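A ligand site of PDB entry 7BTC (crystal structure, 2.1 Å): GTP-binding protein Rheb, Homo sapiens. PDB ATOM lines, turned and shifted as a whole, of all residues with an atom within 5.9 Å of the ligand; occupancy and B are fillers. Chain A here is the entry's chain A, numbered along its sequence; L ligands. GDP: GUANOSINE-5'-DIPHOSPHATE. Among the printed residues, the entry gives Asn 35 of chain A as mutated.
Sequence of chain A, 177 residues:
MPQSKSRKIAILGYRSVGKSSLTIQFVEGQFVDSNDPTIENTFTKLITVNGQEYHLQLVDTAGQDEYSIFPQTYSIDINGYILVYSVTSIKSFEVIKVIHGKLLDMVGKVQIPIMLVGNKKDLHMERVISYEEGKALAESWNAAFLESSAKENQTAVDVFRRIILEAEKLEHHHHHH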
ATOM      1  N   TYR A  14     -19.613  -1.716  36.607  1.00  0.00           N
ATOM      2  CA  TYR A  14     -19.714  -0.264  36.689  1.00  0.00           C
ATOM      3  C   TYR A  14     -21.092   0.180  36.194  1.00  0.00           C
ATOM      4  O   TYR A  14     -21.859  -0.589  35.616  1.00  0.00           O
ATOM      5  CB  TYR A  14     -18.593   0.362  35.872  1.00  0.00           C
ATOM      6  CG  TYR A  14     -18.467   1.877  35.873  1.00  0.00           C
ATOM      7  CD1 TYR A  14     -18.169   2.577  37.042  1.00  0.00           C
ATOM      8  CD2 TYR A  14     -18.546   2.588  34.682  1.00  0.00           C
ATOM      9  CE1 TYR A  14     -18.005   3.967  37.010  1.00  0.00           C
ATOM     10  CE2 TYR A  14     -18.383   3.957  34.640  1.00  0.00           C
ATOM     11  CZ  TYR A  14     -18.113   4.646  35.803  1.00  0.00           C
ATOM     12  OH  TYR A  14     -17.959   6.005  35.732  1.00  0.00           O
ATOM     13  N   ARG A  15     -21.405   1.452  36.432  1.00  0.00           N
ATOM     14  CA  ARG A  15     -22.707   1.955  36.029  1.00  0.00           C
ATOM     15  C   ARG A  15     -22.853   1.931  34.515  1.00  0.00           C
ATOM     16  O   ARG A  15     -21.879   2.112  33.778  1.00  0.00           O
ATOM     17  CB  ARG A  15     -22.926   3.378  36.564  1.00  0.00           C
ATOM     18  N   SER A  16     -24.078   1.674  34.057  1.00  0.00           N
ATOM     19  CA  SER A  16     -24.496   1.794  32.654  1.00  0.00           C
ATOM     20  C   SER A  16     -23.710   0.879  31.717  1.00  0.00           C
ATOM     21  O   SER A  16     -23.578   1.178  30.524  1.00  0.00           O
ATOM     22  CB  SER A  16     -24.400   3.231  32.140  1.00  0.00           C
ATOM     23  OG  SER A  16     -24.738   4.156  33.139  1.00  0.00           O
ATOM     24  N   VAL A  17     -23.221  -0.267  32.208  1.00  0.00           N
ATOM     25  CA  VAL A  17     -22.626  -1.241  31.291  1.00  0.00           C
ATOM     26  C   VAL A  17     -23.657  -2.190  30.696  1.00  0.00           C
ATOM     27  O   VAL A  17     -23.354  -2.882  29.716  1.00  0.00           O
ATOM     28  CB  VAL A  17     -21.494  -2.047  31.973  1.00  0.00           C
ATOM     29  CG1 VAL A  17     -20.374  -1.122  32.434  1.00  0.00           C
ATOM     30  CG2 VAL A  17     -22.027  -2.853  33.151  1.00  0.00           C
ATOM     31  N   GLY A  18     -24.868  -2.236  31.238  1.00  0.00           N
ATOM     32  CA  GLY A  18     -25.899  -3.121  30.731  1.00  0.00           C
ATOM     33  C   GLY A  18     -26.256  -4.270  31.631  1.00  0.00           C
ATOM     34  O   GLY A  18     -26.776  -5.279  31.133  1.00  0.00           O
ATOM     35  N   LYS A  19     -25.991  -4.153  32.937  1.00  0.00           N
ATOM     36  CA  LYS A  19     -26.325  -5.236  33.858  1.00  0.00           C
ATOM     37  C   LYS A  19     -27.826  -5.515  33.821  1.00  0.00           C
ATOM     38  O   LYS A  19     -28.252  -6.649  33.569  1.00  0.00           O
ATOM     39  CB  LYS A  19     -25.856  -4.856  35.270  1.00  0.00           C
ATOM     40  CG  LYS A  19     -24.305  -4.811  35.387  1.00  0.00           C
ATOM     41  CD  LYS A  19     -23.831  -4.505  36.825  1.00  0.00           C
ATOM     42  CE  LYS A  19     -24.452  -3.181  37.352  1.00  0.00           C
ATOM     43  NZ  LYS A  19     -24.069  -1.945  36.575  1.00  0.00           N
ATOM     44  N   SER A  20     -28.639  -4.465  34.004  1.00  0.00           N
ATOM     45  CA  SER A  20     -30.089  -4.612  33.978  1.00  0.00           C
ATOM     46  C   SER A  20     -30.553  -5.093  32.610  1.00  0.00           C
ATOM     47  O   SER A  20     -31.307  -6.078  32.519  1.00  0.00           O
ATOM     48  CB  SER A  20     -30.750  -3.274  34.353  1.00  0.00           C
ATOM     49  OG  SER A  20     -32.155  -3.410  34.432  1.00  0.00           O
ATOM     50  N   SER A  21     -30.096  -4.439  31.528  1.00  0.00           N
ATOM     51  CA  SER A  21     -30.600  -4.778  30.197  1.00  0.00           C
ATOM     52  C   SER A  21     -30.308  -6.227  29.845  1.00  0.00           C
ATOM     53  O   SER A  21     -31.174  -6.927  29.294  1.00  0.00           O
ATOM     54  CB  SER A  21     -29.980  -3.850  29.141  1.00  0.00           C
ATOM     55  OG  SER A  21     -30.401  -2.512  29.291  1.00  0.00           O
ATOM     56  N   LEU A  22     -29.093  -6.688  30.140  1.00  0.00           N
ATOM     57  CA  LEU A  22     -28.728  -8.065  29.833  1.00  0.00           C
ATOM     58  C   LEU A  22     -29.591  -9.047  30.635  1.00  0.00           C
ATOM     59  O   LEU A  22     -30.063 -10.060  30.103  1.00  0.00           O
ATOM     60  CB  LEU A  22     -27.251  -8.284  30.168  1.00  0.00           C
ATOM     61  CG  LEU A  22     -26.292  -9.134  29.364  1.00  0.00           C
ATOM     62  CD1 LEU A  22     -26.511  -9.006  27.856  1.00  0.00           C
ATOM     63  CD2 LEU A  22     -24.887  -8.682  29.764  1.00  0.00           C
ATOM     64  N   PHE A  31     -35.513  -6.291  25.146  1.00  0.00           N
ATOM     65  CA  PHE A  31     -34.530  -5.243  25.371  1.00  0.00           C
ATOM     66  C   PHE A  31     -35.255  -4.018  25.875  1.00  0.00           C
ATOM     67  O   PHE A  31     -36.158  -3.493  25.205  1.00  0.00           O
ATOM     68  CB  PHE A  31     -33.759  -4.924  24.085  1.00  0.00           C
ATOM     69  CG  PHE A  31     -32.829  -3.734  24.205  1.00  0.00           C
ATOM     70  CD1 PHE A  31     -31.683  -3.808  24.972  1.00  0.00           C
ATOM     71  CD2 PHE A  31     -33.117  -2.551  23.548  1.00  0.00           C
ATOM     72  CE1 PHE A  31     -30.835  -2.719  25.074  1.00  0.00           C
ATOM     73  CE2 PHE A  31     -32.275  -1.452  23.658  1.00  0.00           C
ATOM     74  CZ  PHE A  31     -31.125  -1.544  24.423  1.00  0.00           C
ATOM     75  N   VAL A  32     -34.885  -3.557  27.064  1.00  0.00           N
ATOM     76  CA  VAL A  32     -35.471  -2.350  27.659  1.00  0.00           C
ATOM     77  C   VAL A  32     -34.386  -1.291  27.732  1.00  0.00           C
ATOM     78  O   VAL A  32     -33.241  -1.569  28.101  1.00  0.00           O
ATOM     79  CB  VAL A  32     -36.067  -2.642  29.052  1.00  0.00           C
ATOM     80  CG1 VAL A  32     -37.288  -3.538  28.914  1.00  0.00           C
ATOM     81  CG2 VAL A  32     -35.028  -3.287  29.944  1.00  0.00           C
ATOM     82  N   ASP A  33     -34.742  -0.081  27.329  1.00  0.00           N
ATOM     83  CA  ASP A  33     -33.852   1.071  27.377  1.00  0.00           C
ATOM     84  C   ASP A  33     -34.425   2.025  28.418  1.00  0.00           C
ATOM     85  O   ASP A  33     -35.389   2.735  28.151  1.00  0.00           O
ATOM     86  CB  ASP A  33     -33.752   1.728  26.003  1.00  0.00           C
ATOM     87  CG  ASP A  33     -32.755   2.875  25.974  1.00  0.00           C
ATOM     88  OD1 ASP A  33     -32.066   3.097  26.992  1.00  0.00           O
ATOM     89  OD2 ASP A  33     -32.679   3.557  24.929  1.00  0.00           O
ATOM     90  N   SER A  34     -33.816   2.037  29.604  1.00  0.00           N
ATOM     91  CA  SER A  34     -34.338   2.804  30.731  1.00  0.00           C
ATOM     92  C   SER A  34     -33.263   3.710  31.308  1.00  0.00           C
ATOM     93  O   SER A  34     -32.079   3.346  31.347  1.00  0.00           O
ATOM     94  CB  SER A  34     -34.879   1.868  31.821  1.00  0.00           C
ATOM     95  OG  SER A  34     -35.133   2.557  33.032  1.00  0.00           O
ATOM     96  N   ASN A  35     -33.685   4.892  31.747  1.00  0.00           N
ATOM     97  CA  ASN A  35     -32.843   5.870  32.401  1.00  0.00           C
ATOM     98  C   ASN A  35     -32.967   5.840  33.915  1.00  0.00           C
ATOM     99  O   ASN A  35     -32.273   6.604  34.600  1.00  0.00           O
ATOM    100  CB  ASN A  35     -33.171   7.279  31.891  1.00  0.00           C
ATOM    101  CG  ASN A  35     -32.555   7.574  30.539  1.00  0.00           C
ATOM    102  OD1 ASN A  35     -31.631   8.395  30.427  1.00  0.00           O
ATOM    103  ND2 ASN A  35     -33.043   6.899  29.500  1.00  0.00           N
ATOM    104  N   ASP A  36     -33.849   5.006  34.459  1.00  0.00           N
ATOM    105  CA  ASP A  36     -33.813   4.728  35.874  1.00  0.00           C
ATOM    106  C   ASP A  36     -32.440   4.194  36.251  1.00  0.00           C
ATOM    107  O   ASP A  36     -31.882   3.362  35.528  1.00  0.00           O
ATOM    108  CB  ASP A  36     -34.883   3.712  36.256  1.00  0.00           C
ATOM    109  CG  ASP A  36     -36.257   4.319  36.348  1.00  0.00           C
ATOM    110  OD1 ASP A  36     -36.555   5.258  35.567  1.00  0.00           O
ATOM    111  OD2 ASP A  36     -37.054   3.860  37.189  1.00  0.00           O
ATOM    112  N   THR A  38     -29.872   1.761  37.974  1.00  0.00           N
ATOM    113  CA  THR A  38     -29.996   0.356  38.359  1.00  0.00           C
ATOM    114  C   THR A  38     -29.822   0.248  39.875  1.00  0.00           C
ATOM    115  O   THR A  38     -28.796   0.670  40.417  1.00  0.00           O
ATOM    116  CB  THR A  38     -29.000  -0.508  37.614  1.00  0.00           C
ATOM    117  OG1 THR A  38     -29.476  -0.735  36.280  1.00  0.00           O
ATOM    118  CG2 THR A  38     -28.866  -1.849  38.318  1.00  0.00           C
ATOM    119  N   THR A  61     -26.966  -6.010  40.720  1.00  0.00           N
ATOM    120  CA  THR A  61     -26.491  -5.117  41.752  1.00  0.00           C
ATOM    121  C   THR A  61     -26.342  -3.716  41.185  1.00  0.00           C
ATOM    122  O   THR A  61     -26.192  -3.519  39.976  1.00  0.00           O
ATOM    123  CB  THR A  61     -25.165  -5.605  42.319  1.00  0.00           C
ATOM    124  OG1 THR A  61     -24.145  -5.518  41.307  1.00  0.00           O
ATOM    125  CG2 THR A  61     -25.304  -7.040  42.773  1.00  0.00           C
ATOM    126  N   GLY A  63     -24.551  -0.330  40.214  1.00  0.00           N
ATOM    127  CA  GLY A  63     -23.239  -0.163  39.612  1.00  0.00           C
ATOM    128  C   GLY A  63     -22.239   0.320  40.645  1.00  0.00           C
ATOM    129  O   GLY A  63     -22.569   1.134  41.521  1.00  0.00           O
ATOM    130  N   ASN A 119     -19.993  -6.237  27.204  1.00  0.00           N
ATOM    131  CA  ASN A 119     -21.324  -5.992  26.671  1.00  0.00           C
ATOM    132  C   ASN A 119     -21.288  -4.847  25.653  1.00  0.00           C
ATOM    133  O   ASN A 119     -20.287  -4.154  25.487  1.00  0.00           O
ATOM    134  CB  ASN A 119     -22.314  -5.695  27.815  1.00  0.00           C
ATOM    135  CG  ASN A 119     -23.786  -5.641  27.358  1.00  0.00           C
ATOM    136  OD1 ASN A 119     -24.255  -6.487  26.582  1.00  0.00           O
ATOM    137  ND2 ASN A 119     -24.499  -4.656  27.859  1.00  0.00           N
ATOM    138  N   LYS A 120     -22.415  -4.676  24.939  1.00  0.00           N
ATOM    139  CA  LYS A 120     -22.592  -3.636  23.929  1.00  0.00           C
ATOM    140  C   LYS A 120     -21.768  -3.893  22.679  1.00  0.00           C
ATOM    141  O   LYS A 120     -21.348  -2.956  22.009  1.00  0.00           O
ATOM    142  CB  LYS A 120     -22.294  -2.240  24.507  1.00  0.00           C
ATOM    143  CG  LYS A 120     -23.195  -1.887  25.699  1.00  0.00           C
ATOM    144  CD  LYS A 120     -23.164  -0.376  26.018  1.00  0.00           C
ATOM    145  CE  LYS A 120     -23.858  -0.062  27.363  1.00  0.00           C
ATOM    146  NZ  LYS A 120     -23.705   1.357  27.729  1.00  0.00           N
ATOM    147  N   LYS A 121     -21.560  -5.162  22.330  1.00  0.00           N
ATOM    148  CA  LYS A 121     -20.768  -5.463  21.141  1.00  0.00           C
ATOM    149  C   LYS A 121     -21.472  -5.061  19.847  1.00  0.00           C
ATOM    150  O   LYS A 121     -20.840  -5.102  18.787  1.00  0.00           O
ATOM    151  CB  LYS A 121     -20.434  -6.957  21.109  1.00  0.00           C
ATOM    152  CG  LYS A 121     -21.570  -7.814  20.565  1.00  0.00           C
ATOM    153  CD  LYS A 121     -21.368  -9.281  20.873  1.00  0.00           C
ATOM    154  CE  LYS A 121     -21.630 -10.149  19.650  1.00  0.00           C
ATOM    155  NZ  LYS A 121     -22.957  -9.902  19.059  1.00  0.00           N
ATOM    156  N   ASP A 122     -22.759  -4.712  19.910  1.00  0.00           N
ATOM    157  CA  ASP A 122     -23.471  -4.221  18.728  1.00  0.00           C
ATOM    158  C   ASP A 122     -23.062  -2.800  18.337  1.00  0.00           C
ATOM    159  O   ASP A 122     -23.298  -2.403  17.202  1.00  0.00           O
ATOM    160  CB  ASP A 122     -24.980  -4.252  18.967  1.00  0.00           C
ATOM    161  CG  ASP A 122     -25.384  -3.486  20.211  1.00  0.00           C
ATOM    162  OD1 ASP A 122     -25.139  -4.003  21.323  1.00  0.00           O
ATOM    163  OD2 ASP A 122     -25.907  -2.354  20.094  1.00  0.00           O
ATOM    164  N   LEU A 123     -22.461  -2.027  19.248  1.00  0.00           N
ATOM    165  CA  LEU A 123     -22.072  -0.636  18.956  1.00  0.00           C
ATOM    166  C   LEU A 123     -20.657  -0.588  18.364  1.00  0.00           C
ATOM    167  O   LEU A 123     -19.687  -0.145  18.986  1.00  0.00           O
ATOM    168  CB  LEU A 123     -22.174   0.230  20.202  1.00  0.00           C
ATOM    169  CG  LEU A 123     -23.561   0.228  20.841  1.00  0.00           C
ATOM    170  CD1 LEU A 123     -23.551   1.064  22.107  1.00  0.00           C
ATOM    171  CD2 LEU A 123     -24.609   0.722  19.837  1.00  0.00           C
ATOM    172  N   SER A 148     -21.149  -9.736  24.533  1.00  0.00           N
ATOM    173  CA  SER A 148     -22.603  -9.831  24.471  1.00  0.00           C
ATOM    174  C   SER A 148     -23.206  -8.535  23.954  1.00  0.00           C
ATOM    175  O   SER A 148     -22.540  -7.499  23.838  1.00  0.00           O
ATOM    176  CB  SER A 148     -23.225 -10.148  25.842  1.00  0.00           C
ATOM    177  OG  SER A 148     -22.990  -9.099  26.733  1.00  0.00           O
ATOM    178  N   SER A 149     -24.502  -8.615  23.655  1.00  0.00           N
ATOM    179  CA  SER A 149     -25.319  -7.443  23.403  1.00  0.00           C
ATOM    180  C   SER A 149     -26.689  -7.717  24.019  1.00  0.00           C
ATOM    181  O   SER A 149     -27.324  -8.725  23.698  1.00  0.00           O
ATOM    182  CB  SER A 149     -25.436  -7.144  21.905  1.00  0.00           C
ATOM    183  OG  SER A 149     -26.477  -6.211  21.631  1.00  0.00           O
ATOM    184  N   ALA A 150     -27.112  -6.823  24.922  1.00  0.00           N
ATOM    185  CA  ALA A 150     -28.456  -6.901  25.489  1.00  0.00           C
ATOM    186  C   ALA A 150     -29.560  -6.800  24.427  1.00  0.00           C
ATOM    187  O   ALA A 150     -30.719  -7.086  24.733  1.00  0.00           O
ATOM    188  CB  ALA A 150     -28.667  -5.778  26.507  1.00  0.00           C
ATOM    189  N   LYS A 151     -29.230  -6.372  23.200  1.00  0.00           N
ATOM    190  CA  LYS A 151     -30.211  -6.358  22.114  1.00  0.00           C
ATOM    191  C   LYS A 151     -30.371  -7.711  21.449  1.00  0.00           C
ATOM    192  O   LYS A 151     -31.272  -7.879  20.618  1.00  0.00           O
ATOM    193  CB  LYS A 151     -29.812  -5.348  21.041  1.00  0.00           C
ATOM    194  CG  LYS A 151     -29.776  -3.906  21.516  1.00  0.00           C
ATOM    195  CD  LYS A 151     -29.775  -2.966  20.317  1.00  0.00           C
ATOM    196  CE  LYS A 151     -29.944  -1.518  20.742  1.00  0.00           C
ATOM    197  NZ  LYS A 151     -30.123  -0.620  19.571  1.00  0.00           N
HETATM  198  PB  GDP L   1     -26.640  -0.883  34.175  1.00  0.00           P
HETATM  199  O1B GDP L   1     -25.321  -1.668  34.175  1.00  0.00           O
HETATM  200  O2B GDP L   1     -26.401   0.384  34.958  1.00  0.00           O
HETATM  201  O3B GDP L   1     -27.718  -1.746  34.757  1.00  0.00           O
HETATM  202  O3A GDP L   1     -26.888  -0.535  32.626  1.00  0.00           O
HETATM  203  PA  GDP L   1     -28.295  -0.507  31.823  1.00  0.00           P
HETATM  204  O1A GDP L   1     -28.837  -1.872  31.504  1.00  0.00           O
HETATM  205  O2A GDP L   1     -29.253   0.405  32.526  1.00  0.00           O
HETATM  206  O5' GDP L   1     -27.777   0.142  30.447  1.00  0.00           O
HETATM  207  C5' GDP L   1     -27.340   1.499  30.411  1.00  0.00           C
HETATM  208  C4' GDP L   1     -27.675   2.031  29.037  1.00  0.00           C
HETATM  209  O4' GDP L   1     -27.043   1.242  28.032  1.00  0.00           O
HETATM  210  C3' GDP L   1     -29.176   1.914  28.748  1.00  0.00           C
HETATM  211  O3' GDP L   1     -29.481   2.974  27.855  1.00  0.00           O
HETATM  212  C2' GDP L   1     -29.326   0.663  27.923  1.00  0.00           C
HETATM  213  O2' GDP L   1     -30.456   0.762  27.049  1.00  0.00           O
HETATM  214  C1' GDP L   1     -28.011   0.631  27.144  1.00  0.00           C
HETATM  215  N9  GDP L   1     -27.513  -0.722  26.834  1.00  0.00           N
HETATM  216  C8  GDP L   1     -27.280  -1.703  27.745  1.00  0.00           C
HETATM  217  N7  GDP L   1     -26.801  -2.820  27.136  1.00  0.00           N
HETATM  218  C5  GDP L   1     -26.687  -2.542  25.820  1.00  0.00           C
HETATM  219  C6  GDP L   1     -26.208  -3.284  24.629  1.00  0.00           C
HETATM  220  O6  GDP L   1     -25.807  -4.460  24.731  1.00  0.00           O
HETATM  221  N1  GDP L   1     -26.254  -2.652  23.453  1.00  0.00           N
HETATM  222  C2  GDP L   1     -26.701  -1.389  23.310  1.00  0.00           C
HETATM  223  N2  GDP L   1     -26.705  -0.834  22.063  1.00  0.00           N
HETATM  224  N3  GDP L   1     -27.124  -0.647  24.366  1.00  0.00           N
HETATM  225  C4  GDP L   1     -27.134  -1.164  25.620  1.00  0.00           C
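The side-chain hydroxyl (OG1) of Thr 38 is in hydrogen-bond range of an oxygen (O3B) of the ligand (2.5 Å). The backbone NH of Ala 150 sits at hydrogen-bond distance from an oxygen (O6) of the ligand. The backbone NH of Lys 19 sits at hydrogen-bond distance from an oxygen (O1B) of the ligand (2.9 Å). NZ of Lys 120 lies within hydrogen-bond range of O4' of the ligand, at 3.4 Å. A nitrogen (N7) of the ligand lies within hydrogen-bond range of the side-chain amide nitrogen (ND2) of Asn 119, 3.0 Å away. The side-chain carboxylate of Asp 122 is in hydrogen-bond range of a nitrogen (N2) of the ligand. N of Gly 18 lies within hydrogen-bond range of O3A of the ligand (3.0 Å). The side-chain carboxylate (OD1) of Asp 33 sits at hydrogen-bond distance from an oxygen (O3') of the ligand, at 2.7 Å. O1A of the ligand sits at hydrogen-bond distance from OG of Ser 21, at 2.8 Å. An oxygen (O6) of the ligand lies within hydrogen-bond range of the backbone NH (N) of Lys 120 (3.4 Å). An oxygen (O1B) of the ligand is in salt-bridge range of the side-chain amino group (NZ) of Lys 19, 2.7 Å away. N of Val 17 is in hydrogen-bond range of O1B of the ligand, at 3.2 Å. An oxygen (O1A) of the ligand lies within hydrogen-bond range of the backbone NH (N) of Ser 21 (2.9 Å). N of Ser 20 sits at hydrogen-bond distance from O3B of the ligand (3.0 Å). O2B of the ligand lies within hydrogen-bond range of N of Ser 16, at 2.8 Å.
OD1 of Asn 119 sits at hydrogen-bond distance from N of Ala 150 (3.3 Å). The side-chain hydroxyl of Ser 148 sits at hydrogen-bond distance from the side-chain amide oxygen of Asn 119, 2.9 Å away. OD1 of Asp 122 is in hydrogen-bond range of OG of Ser 149 (2.6 Å). N of Lys 120 lies within hydrogen-bond range of O of Ser 148 (3.0 Å). O of Tyr 14 lies within hydrogen-bond range of NZ of Lys 19 (2.8 Å). The side-chain hydroxyl of Ser 21 is in hydrogen-bond range of the backbone carbonyl oxygen of Val 32 (3.2 Å). The side-chain amide nitrogen (ND2) of Asn 119 is in hydrogen-bond range of the backbone carbonyl oxygen (O) of Val 17 (2.8 Å). The backbone carbonyl oxygen of Ser 16 is in hydrogen-bond range of the side-chain amino group of Lys 120.
Residues that only touch the ligand: Tyr 14 (3.9 Å), Arg 15 (3.9 Å), Phe 31 (3.6 Å), Val 32 (3.8 Å), Leu 123 (3.4 Å), Ser 149 (3.3 Å) and Lys 151 (3.6 Å). 19 residues have an atom within 4 Å of the ligand: Tyr 14, Arg 15, Ser 16, Val 17, Gly 18, Lys 19, Ser 20, Ser 21, Phe 31, Val 32, Asp 33, Thr 38, Asn 119, Lys 120, Asp 122, Leu 123, Ser 149, Ala 150 and Lys 151.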
